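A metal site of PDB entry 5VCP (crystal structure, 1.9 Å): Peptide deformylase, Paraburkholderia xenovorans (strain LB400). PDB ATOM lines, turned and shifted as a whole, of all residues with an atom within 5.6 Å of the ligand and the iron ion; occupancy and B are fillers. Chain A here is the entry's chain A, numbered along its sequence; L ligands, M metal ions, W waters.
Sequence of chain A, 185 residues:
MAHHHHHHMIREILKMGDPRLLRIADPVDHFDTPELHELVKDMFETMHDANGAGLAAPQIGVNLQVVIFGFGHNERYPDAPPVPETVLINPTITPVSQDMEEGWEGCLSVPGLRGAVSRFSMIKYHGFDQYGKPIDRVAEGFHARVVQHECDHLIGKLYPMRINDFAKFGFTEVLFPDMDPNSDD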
ATOM      1  N   ALA A  50     -23.597 -31.481  -3.714  1.00  0.00           N
ATOM      2  CA  ALA A  50     -22.713 -30.329  -3.557  1.00  0.00           C
ATOM      3  C   ALA A  50     -23.162 -29.385  -2.424  1.00  0.00           C
ATOM      4  O   ALA A  50     -22.581 -28.314  -2.236  1.00  0.00           O
ATOM      5  CB  ALA A  50     -22.623 -29.558  -4.868  1.00  0.00           C
ATOM      6  N   ASN A  51     -24.198 -29.795  -1.688  1.00  0.00           N
ATOM      7  CA  ASN A  51     -24.779 -28.981  -0.618  1.00  0.00           C
ATOM      8  C   ASN A  51     -25.227 -27.584  -1.054  1.00  0.00           C
ATOM      9  O   ASN A  51     -25.010 -26.612  -0.316  1.00  0.00           O
ATOM     10  CB  ASN A  51     -23.806 -28.855   0.557  1.00  0.00           C
ATOM     11  CG  ASN A  51     -23.567 -30.178   1.253  1.00  0.00           C
ATOM     12  OD1 ASN A  51     -24.433 -30.674   1.968  1.00  0.00           O
ATOM     13  ND2 ASN A  51     -22.391 -30.759   1.046  1.00  0.00           N
ATOM     14  N   GLY A  52     -25.841 -27.483  -2.227  1.00  0.00           N
ATOM     15  CA  GLY A  52     -26.286 -26.203  -2.736  1.00  0.00           C
ATOM     16  C   GLY A  52     -27.705 -25.804  -2.366  1.00  0.00           C
ATOM     17  O   GLY A  52     -28.534 -26.668  -2.082  1.00  0.00           O
ATOM     18  N   ALA A  53     -27.998 -24.514  -2.388  1.00  0.00           N
ATOM     19  CA  ALA A  53     -29.363 -24.041  -2.140  1.00  0.00           C
ATOM     20  C   ALA A  53     -30.163 -23.934  -3.442  1.00  0.00           C
ATOM     21  O   ALA A  53     -31.367 -23.682  -3.416  1.00  0.00           O
ATOM     22  CB  ALA A  53     -29.345 -22.709  -1.450  1.00  0.00           C
ATOM     23  N   GLY A  54     -29.484 -24.106  -4.576  1.00  0.00           N
ATOM     24  CA  GLY A  54     -30.137 -24.011  -5.865  1.00  0.00           C
ATOM     25  C   GLY A  54     -29.245 -24.534  -6.979  1.00  0.00           C
ATOM     26  O   GLY A  54     -28.061 -24.784  -6.766  1.00  0.00           O
ATOM     27  N   LEU A  55     -29.813 -24.707  -8.161  1.00  0.00           N
ATOM     28  CA  LEU A  55     -29.028 -25.125  -9.323  1.00  0.00           C
ATOM     29  C   LEU A  55     -29.779 -24.789 -10.585  1.00  0.00           C
ATOM     30  O   LEU A  55     -31.003 -24.850 -10.626  1.00  0.00           O
ATOM     31  CB  LEU A  55     -28.721 -26.629  -9.285  1.00  0.00           C
ATOM     32  CG  LEU A  55     -27.589 -27.121 -10.193  1.00  0.00           C
ATOM     33  CD1 LEU A  55     -26.256 -26.775  -9.515  1.00  0.00           C
ATOM     34  CD2 LEU A  55     -27.679 -28.628 -10.450  1.00  0.00           C
ATOM     35  N   ALA A  56     -29.042 -24.395 -11.612  1.00  0.00           N
ATOM     36  CA  ALA A  56     -29.652 -24.091 -12.907  1.00  0.00           C
ATOM     37  C   ALA A  56     -29.152 -25.081 -13.961  1.00  0.00           C
ATOM     38  O   ALA A  56     -27.977 -25.463 -13.971  1.00  0.00           O
ATOM     39  CB  ALA A  56     -29.325 -22.636 -13.318  1.00  0.00           C
ATOM     40  N   GLN A  59     -25.689 -25.140 -15.557  1.00  0.00           N
ATOM     41  CA  GLN A  59     -24.569 -25.530 -14.706  1.00  0.00           C
ATOM     42  C   GLN A  59     -24.201 -27.017 -14.854  1.00  0.00           C
ATOM     43  O   GLN A  59     -23.134 -27.423 -14.415  1.00  0.00           O
ATOM     44  CB  GLN A  59     -24.864 -25.228 -13.224  1.00  0.00           C
ATOM     45  CG  GLN A  59     -24.820 -23.757 -12.869  1.00  0.00           C
ATOM     46  CD  GLN A  59     -25.171 -23.539 -11.433  1.00  0.00           C
ATOM     47  OE1 GLN A  59     -26.346 -23.634 -11.044  1.00  0.00           O
ATOM     48  NE2 GLN A  59     -24.165 -23.298 -10.605  1.00  0.00           N
ATOM     49  N   TRP A 104     -23.920 -11.013   0.364  1.00  0.00           N
ATOM     50  CA  TRP A 104     -22.850 -11.903  -0.078  1.00  0.00           C
ATOM     51  C   TRP A 104     -23.410 -13.111  -0.841  1.00  0.00           C
ATOM     52  O   TRP A 104     -24.369 -13.733  -0.398  1.00  0.00           O
ATOM     53  CB  TRP A 104     -22.019 -12.367   1.110  1.00  0.00           C
ATOM     54  CG  TRP A 104     -21.193 -11.247   1.677  1.00  0.00           C
ATOM     55  CD1 TRP A 104     -21.453 -10.532   2.798  1.00  0.00           C
ATOM     56  CD2 TRP A 104     -19.986 -10.700   1.120  1.00  0.00           C
ATOM     57  NE1 TRP A 104     -20.481  -9.572   2.987  1.00  0.00           N
ATOM     58  CE2 TRP A 104     -19.566  -9.664   1.969  1.00  0.00           C
ATOM     59  CE3 TRP A 104     -19.213 -11.009  -0.009  1.00  0.00           C
ATOM     60  CZ2 TRP A 104     -18.404  -8.915   1.730  1.00  0.00           C
ATOM     61  CZ3 TRP A 104     -18.057 -10.272  -0.245  1.00  0.00           C
ATOM     62  CH2 TRP A 104     -17.680  -9.231   0.621  1.00  0.00           C
ATOM     63  N   GLU A 105     -22.810 -13.434  -1.980  1.00  0.00           N
ATOM     64  CA  GLU A 105     -23.215 -14.593  -2.765  1.00  0.00           C
ATOM     65  C   GLU A 105     -22.036 -15.477  -3.099  1.00  0.00           C
ATOM     66  O   GLU A 105     -20.917 -14.997  -3.225  1.00  0.00           O
ATOM     67  CB  GLU A 105     -23.902 -14.162  -4.067  1.00  0.00           C
ATOM     68  CG  GLU A 105     -25.153 -13.358  -3.849  1.00  0.00           C
ATOM     69  CD  GLU A 105     -25.970 -13.170  -5.112  1.00  0.00           C
ATOM     70  OE1 GLU A 105     -25.657 -13.791  -6.159  1.00  0.00           O
ATOM     71  OE2 GLU A 105     -26.960 -12.411  -5.046  1.00  0.00           O
ATOM     72  N   GLY A 106     -22.303 -16.760  -3.205  1.00  0.00           N
ATOM     73  CA  GLY A 106     -21.361 -17.708  -3.762  1.00  0.00           C
ATOM     74  C   GLY A 106     -22.125 -18.546  -4.787  1.00  0.00           C
ATOM     75  O   GLY A 106     -23.353 -18.450  -4.872  1.00  0.00           O
ATOM     76  N   CYS A 107     -21.403 -19.352  -5.558  1.00  0.00           N
ATOM     77  CA  CYS A 107     -21.974 -20.151  -6.648  1.00  0.00           C
ATOM     78  C   CYS A 107     -21.182 -21.449  -6.743  1.00  0.00           C
ATOM     79  O   CYS A 107     -19.957 -21.426  -6.584  1.00  0.00           O
ATOM     80  CB  CYS A 107     -21.926 -19.354  -7.955  1.00  0.00           C
ATOM     81  SG  CYS A 107     -22.457 -20.205  -9.479  1.00  0.00           S
ATOM     82  N   LEU A 108     -21.855 -22.567  -6.975  1.00  0.00           N
ATOM     83  CA  LEU A 108     -21.180 -23.852  -7.135  1.00  0.00           C
ATOM     84  C   LEU A 108     -20.264 -23.827  -8.367  1.00  0.00           C
ATOM     85  O   LEU A 108     -19.321 -24.620  -8.460  1.00  0.00           O
ATOM     86  CB  LEU A 108     -22.194 -24.996  -7.235  1.00  0.00           C
ATOM     87  CG  LEU A 108     -23.069 -25.209  -5.991  1.00  0.00           C
ATOM     88  CD1 LEU A 108     -24.183 -26.213  -6.280  1.00  0.00           C
ATOM     89  CD2 LEU A 108     -22.229 -25.656  -4.815  1.00  0.00           C
ATOM     90  N   SER A 109     -20.551 -22.948  -9.320  1.00  0.00           N
ATOM     91  CA  SER A 109     -19.697 -22.842 -10.488  1.00  0.00           C
ATOM     92  C   SER A 109     -18.484 -21.924 -10.211  1.00  0.00           C
ATOM     93  O   SER A 109     -17.570 -21.839 -11.020  1.00  0.00           O
ATOM     94  CB  SER A 109     -20.510 -22.325 -11.690  1.00  0.00           C
ATOM     95  OG  SER A 109     -21.547 -23.252 -12.026  1.00  0.00           O
ATOM     96  N   ARG A 114     -16.499 -15.572  -2.700  1.00  0.00           N
ATOM     97  CA  ARG A 114     -17.733 -14.858  -2.365  1.00  0.00           C
ATOM     98  C   ARG A 114     -17.640 -13.438  -2.903  1.00  0.00           C
ATOM     99  O   ARG A 114     -16.548 -12.875  -2.981  1.00  0.00           O
ATOM    100  CB  ARG A 114     -17.960 -14.820  -0.849  1.00  0.00           C
ATOM    101  CG  ARG A 114     -18.161 -16.189  -0.179  1.00  0.00           C
ATOM    102  CD  ARG A 114     -19.520 -16.783  -0.464  1.00  0.00           C
ATOM    103  NE  ARG A 114     -19.764 -17.990   0.317  1.00  0.00           N
ATOM    104  CZ  ARG A 114     -19.426 -19.231  -0.065  1.00  0.00           C
ATOM    105  NH1 ARG A 114     -18.815 -19.433  -1.229  1.00  0.00           N
ATOM    106  NH2 ARG A 114     -19.692 -20.262   0.724  1.00  0.00           N
ATOM    107  N   PHE A 142     -33.752 -13.276   1.098  1.00  0.00           N
ATOM    108  CA  PHE A 142     -32.942 -14.393   0.596  1.00  0.00           C
ATOM    109  C   PHE A 142     -33.657 -15.221  -0.472  1.00  0.00           C
ATOM    110  O   PHE A 142     -33.059 -15.609  -1.473  1.00  0.00           O
ATOM    111  CB  PHE A 142     -32.506 -15.297   1.764  1.00  0.00           C
ATOM    112  CG  PHE A 142     -31.508 -16.335   1.367  1.00  0.00           C
ATOM    113  CD1 PHE A 142     -30.232 -15.969   0.948  1.00  0.00           C
ATOM    114  CD2 PHE A 142     -31.840 -17.669   1.381  1.00  0.00           C
ATOM    115  CE1 PHE A 142     -29.316 -16.931   0.562  1.00  0.00           C
ATOM    116  CE2 PHE A 142     -30.924 -18.631   0.995  1.00  0.00           C
ATOM    117  CZ  PHE A 142     -29.658 -18.265   0.586  1.00  0.00           C
ATOM    118  N   ARG A 145     -33.392 -13.377  -3.561  1.00  0.00           N
ATOM    119  CA  ARG A 145     -32.003 -13.423  -4.014  1.00  0.00           C
ATOM    120  C   ARG A 145     -31.679 -14.746  -4.730  1.00  0.00           C
ATOM    121  O   ARG A 145     -31.108 -14.735  -5.824  1.00  0.00           O
ATOM    122  CB  ARG A 145     -31.056 -13.224  -2.840  1.00  0.00           C
ATOM    123  CG  ARG A 145     -29.576 -13.333  -3.169  1.00  0.00           C
ATOM    124  CD  ARG A 145     -28.740 -12.916  -1.961  1.00  0.00           C
ATOM    125  NE  ARG A 145     -28.990 -11.531  -1.553  1.00  0.00           N
ATOM    126  CZ  ARG A 145     -28.346 -10.469  -2.048  1.00  0.00           C
ATOM    127  NH1 ARG A 145     -27.394 -10.615  -2.960  1.00  0.00           N
ATOM    128  NH2 ARG A 145     -28.633  -9.252  -1.600  1.00  0.00           N
ATOM    129  N   VAL A 146     -32.053 -15.885  -4.126  1.00  0.00           N
ATOM    130  CA  VAL A 146     -31.775 -17.185  -4.747  1.00  0.00           C
ATOM    131  C   VAL A 146     -32.436 -17.286  -6.107  1.00  0.00           C
ATOM    132  O   VAL A 146     -31.848 -17.774  -7.072  1.00  0.00           O
ATOM    133  CB  VAL A 146     -32.217 -18.352  -3.850  1.00  0.00           C
ATOM    134  CG1 VAL A 146     -32.065 -19.685  -4.585  1.00  0.00           C
ATOM    135  CG2 VAL A 146     -31.397 -18.345  -2.551  1.00  0.00           C
ATOM    136  N   HIS A 149     -30.542 -15.106  -8.553  1.00  0.00           N
ATOM    137  CA  HIS A 149     -29.268 -15.764  -8.826  1.00  0.00           C
ATOM    138  C   HIS A 149     -29.428 -16.928  -9.827  1.00  0.00           C
ATOM    139  O   HIS A 149     -28.669 -17.053 -10.803  1.00  0.00           O
ATOM    140  CB  HIS A 149     -28.668 -16.248  -7.503  1.00  0.00           C
ATOM    141  CG  HIS A 149     -27.326 -16.912  -7.650  1.00  0.00           C
ATOM    142  ND1 HIS A 149     -26.159 -16.317  -7.197  1.00  0.00           N
ATOM    143  CD2 HIS A 149     -26.966 -18.117  -8.145  1.00  0.00           C
ATOM    144  CE1 HIS A 149     -25.150 -17.131  -7.426  1.00  0.00           C
ATOM    145  NE2 HIS A 149     -25.611 -18.226  -8.005  1.00  0.00           N
ATOM    146  N   GLU A 150     -30.408 -17.804  -9.581  1.00  0.00           N
ATOM    147  CA  GLU A 150     -30.602 -18.964 -10.471  1.00  0.00           C
ATOM    148  C   GLU A 150     -31.036 -18.545 -11.864  1.00  0.00           C
ATOM    149  O   GLU A 150     -30.516 -19.064 -12.859  1.00  0.00           O
ATOM    150  CB  GLU A 150     -31.632 -19.960  -9.897  1.00  0.00           C
ATOM    151  CG  GLU A 150     -31.239 -20.590  -8.580  1.00  0.00           C
ATOM    152  CD  GLU A 150     -29.844 -21.189  -8.611  1.00  0.00           C
ATOM    153  OE1 GLU A 150     -29.360 -21.597  -9.694  1.00  0.00           O
ATOM    154  OE2 GLU A 150     -29.218 -21.270  -7.540  1.00  0.00           O
ATOM    155  N   HIS A 153     -28.365 -17.372 -14.310  1.00  0.00           N
ATOM    156  CA  HIS A 153     -27.702 -18.437 -15.069  1.00  0.00           C
ATOM    157  C   HIS A 153     -28.353 -18.695 -16.431  1.00  0.00           C
ATOM    158  O   HIS A 153     -27.673 -19.072 -17.385  1.00  0.00           O
ATOM    159  CB  HIS A 153     -27.725 -19.756 -14.324  1.00  0.00           C
ATOM    160  CG  HIS A 153     -26.663 -19.870 -13.269  1.00  0.00           C
ATOM    161  ND1 HIS A 153     -25.325 -19.831 -13.573  1.00  0.00           N
ATOM    162  CD2 HIS A 153     -26.751 -20.000 -11.928  1.00  0.00           C
ATOM    163  CE1 HIS A 153     -24.623 -19.951 -12.460  1.00  0.00           C
ATOM    164  NE2 HIS A 153     -25.463 -20.046 -11.445  1.00  0.00           N
ATOM    165  N   PHE A 176     -14.262 -14.685   5.448  1.00  0.00           N
ATOM    166  CA  PHE A 176     -15.003 -15.240   6.573  1.00  0.00           C
ATOM    167  C   PHE A 176     -14.225 -16.350   7.278  1.00  0.00           C
ATOM    168  O   PHE A 176     -14.522 -17.532   7.093  1.00  0.00           O
ATOM    169  CB  PHE A 176     -16.372 -15.781   6.119  1.00  0.00           C
ATOM    170  CG  PHE A 176     -17.196 -14.774   5.348  1.00  0.00           C
ATOM    171  CD1 PHE A 176     -17.863 -13.758   6.000  1.00  0.00           C
ATOM    172  CD2 PHE A 176     -17.285 -14.854   3.961  1.00  0.00           C
ATOM    173  CE1 PHE A 176     -18.621 -12.828   5.296  1.00  0.00           C
ATOM    174  CE2 PHE A 176     -18.031 -13.924   3.247  1.00  0.00           C
ATOM    175  CZ  PHE A 176     -18.701 -12.912   3.907  1.00  0.00           C
HETATM  176  C1  LIG L   1     -25.972 -22.419  -5.657  1.00  0.00           C
HETATM  177  C2  LIG L   1     -25.772 -22.139  -7.126  1.00  0.00           C
HETATM  178  O1  LIG L   1     -24.657 -22.142  -7.638  1.00  0.00           O
HETATM  179  N1  LIG L   1     -26.888 -21.889  -7.797  1.00  0.00           N
HETATM  180  O2  LIG L   1     -26.828 -21.667  -9.165  1.00  0.00           O
HETATM  181  C3  LIG L   1     -26.044 -21.147  -4.811  1.00  0.00           C
HETATM  182  C4  LIG L   1     -25.687 -21.504  -3.391  1.00  0.00           C
HETATM  183  O3  LIG L   1     -26.171 -22.486  -2.830  1.00  0.00           O
HETATM  184  C5  LIG L   1     -27.462 -20.556  -4.846  1.00  0.00           C
HETATM  185  C6  LIG L   1     -27.668 -19.314  -3.986  1.00  0.00           C
HETATM  186  C7  LIG L   1     -26.902 -18.090  -4.473  1.00  0.00           C
HETATM  187  C8  LIG L   1     -27.108 -16.846  -3.635  1.00  0.00           C
HETATM  188  C9  LIG L   1     -26.659 -17.029  -2.218  1.00  0.00           C
HETATM  189  N2  LIG L   1     -24.810 -20.672  -2.817  1.00  0.00           N
HETATM  190  C10 LIG L   1     -24.422 -20.759  -1.420  1.00  0.00           C
HETATM  191  C11 LIG L   1     -23.101 -21.535  -1.238  1.00  0.00           C
HETATM  192  C12 LIG L   1     -21.951 -20.874  -1.989  1.00  0.00           C
HETATM  193  C13 LIG L   1     -23.223 -22.994  -1.638  1.00  0.00           C
HETATM  194  C14 LIG L   1     -24.283 -19.328  -0.916  1.00  0.00           C
HETATM  195  O4  LIG L   1     -23.917 -18.447  -1.682  1.00  0.00           O
HETATM  196  N3  LIG L   1     -24.608 -19.060   0.357  1.00  0.00           N
HETATM  197  C15 LIG L   1     -24.477 -17.688   0.897  1.00  0.00           C
HETATM  198  C16 LIG L   1     -25.159 -19.979   1.364  1.00  0.00           C
HETATM  199  C17 LIG L   1     -26.033 -19.083   2.195  1.00  0.00           C
HETATM  200  C18 LIG L   1     -25.316 -17.732   2.181  1.00  0.00           C
HETATM  201  C19 LIG L   1     -23.018 -17.331   1.146  1.00  0.00           C
HETATM  202  O5  LIG L   1     -22.860 -15.960   1.495  1.00  0.00           O
HETATM  203 FE    FE M   1     -24.834 -20.092  -9.225  1.00  0.00          FE
HETATM  204  O   HOH W   1     -23.593 -17.087 -10.344  1.00  0.00           O
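The side-chain carboxylate of Glu 150 lies within hydrogen-bond range of a nitrogen (N1) of the ligand, at 2.4 Å. The side-chain amide oxygen of Gln 59 sits close to an oxygen (O2) of the ligand, at 2.8 Å. An oxygen (O3) of the ligand lies within hydrogen-bond range of the backbone NH of Ala 53 (2.8 Å). The backbone NH (N) of Gly 106 lies within hydrogen-bond range of an oxygen (O4) of the ligand. O of Gly 106 sits at hydrogen-bond distance from N2 of the ligand, 3.4 Å away. An oxygen (O1) of the ligand lies close to the backbone NH of Leu 108 (2.9 Å). The backbone carbonyl oxygen of Gly 54 sits at hydrogen-bond distance from a nitrogen (N1) of the ligand (3.3 Å). O5 of the ligand is in hydrogen-bond range of O of Trp 104 (3.3 Å).
ND1 of His 149 is in hydrogen-bond range of OE1 of Glu 105, 2.8 Å away. The side-chain sulfur of Cys 107 lies close to the side-chain amide nitrogen of Gln 59, 3.7 Å away. N of Ser 109 lies close to SG of Cys 107 (3.3 Å). OE1 of Glu 150 sits close to N of Leu 55 (3.5 Å). OE1 of Glu 150 is in hydrogen-bond range of N of Ala 56, 3.4 Å away. The backbone NH (N) of Ala 56 is in hydrogen-bond range of the side-chain amide oxygen (OE1) of Gln 59 (2.9 Å). The side-chain amide nitrogen of Gln 59 is in hydrogen-bond range of the side-chain hydroxyl of Ser 109 (3.0 Å). The side-chain carboxylate (OE2) of Glu 105 is in salt-bridge range of the guanidinium group (NH1) of Arg 145, at 2.8 Å.
Gly 52 touches the ligand (C to O3, 3.7 Å). Glu 105 touches the ligand. Arg 114 touches the ligand (NE to C19, 3.4 Å). Phe 142 touches the ligand. Hydrophobic or aromatic side chains that line the ligand: Ala 53, Trp 104, Leu 108, Phe 142, His 149 and His 153. Within 4 Å of the ligand: Gly 52, Ala 53, Gly 54, Gln 59, Trp 104, Glu 105, Gly 106, Cys 107, Leu 108, Arg 114, Phe 142, His 149, Glu 150 and His 153. The nearest printed residue that does not touch the ligand is Leu 55 (4.1 Å).
Merely in contact with the iron ion: Gln 59. Four residues have an atom within 4 Å of the iron ion: Gln 59, Cys 107, His 149 and His 153.
The iron ion is bound by NE2 of His 153 (2.3 Å), NE2 of His 149 (2.4 Å), SG of Cys 107 (2.4 Å), O2 of the ligand (2.5 Å) and O1 of the ligand (2.6 Å).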
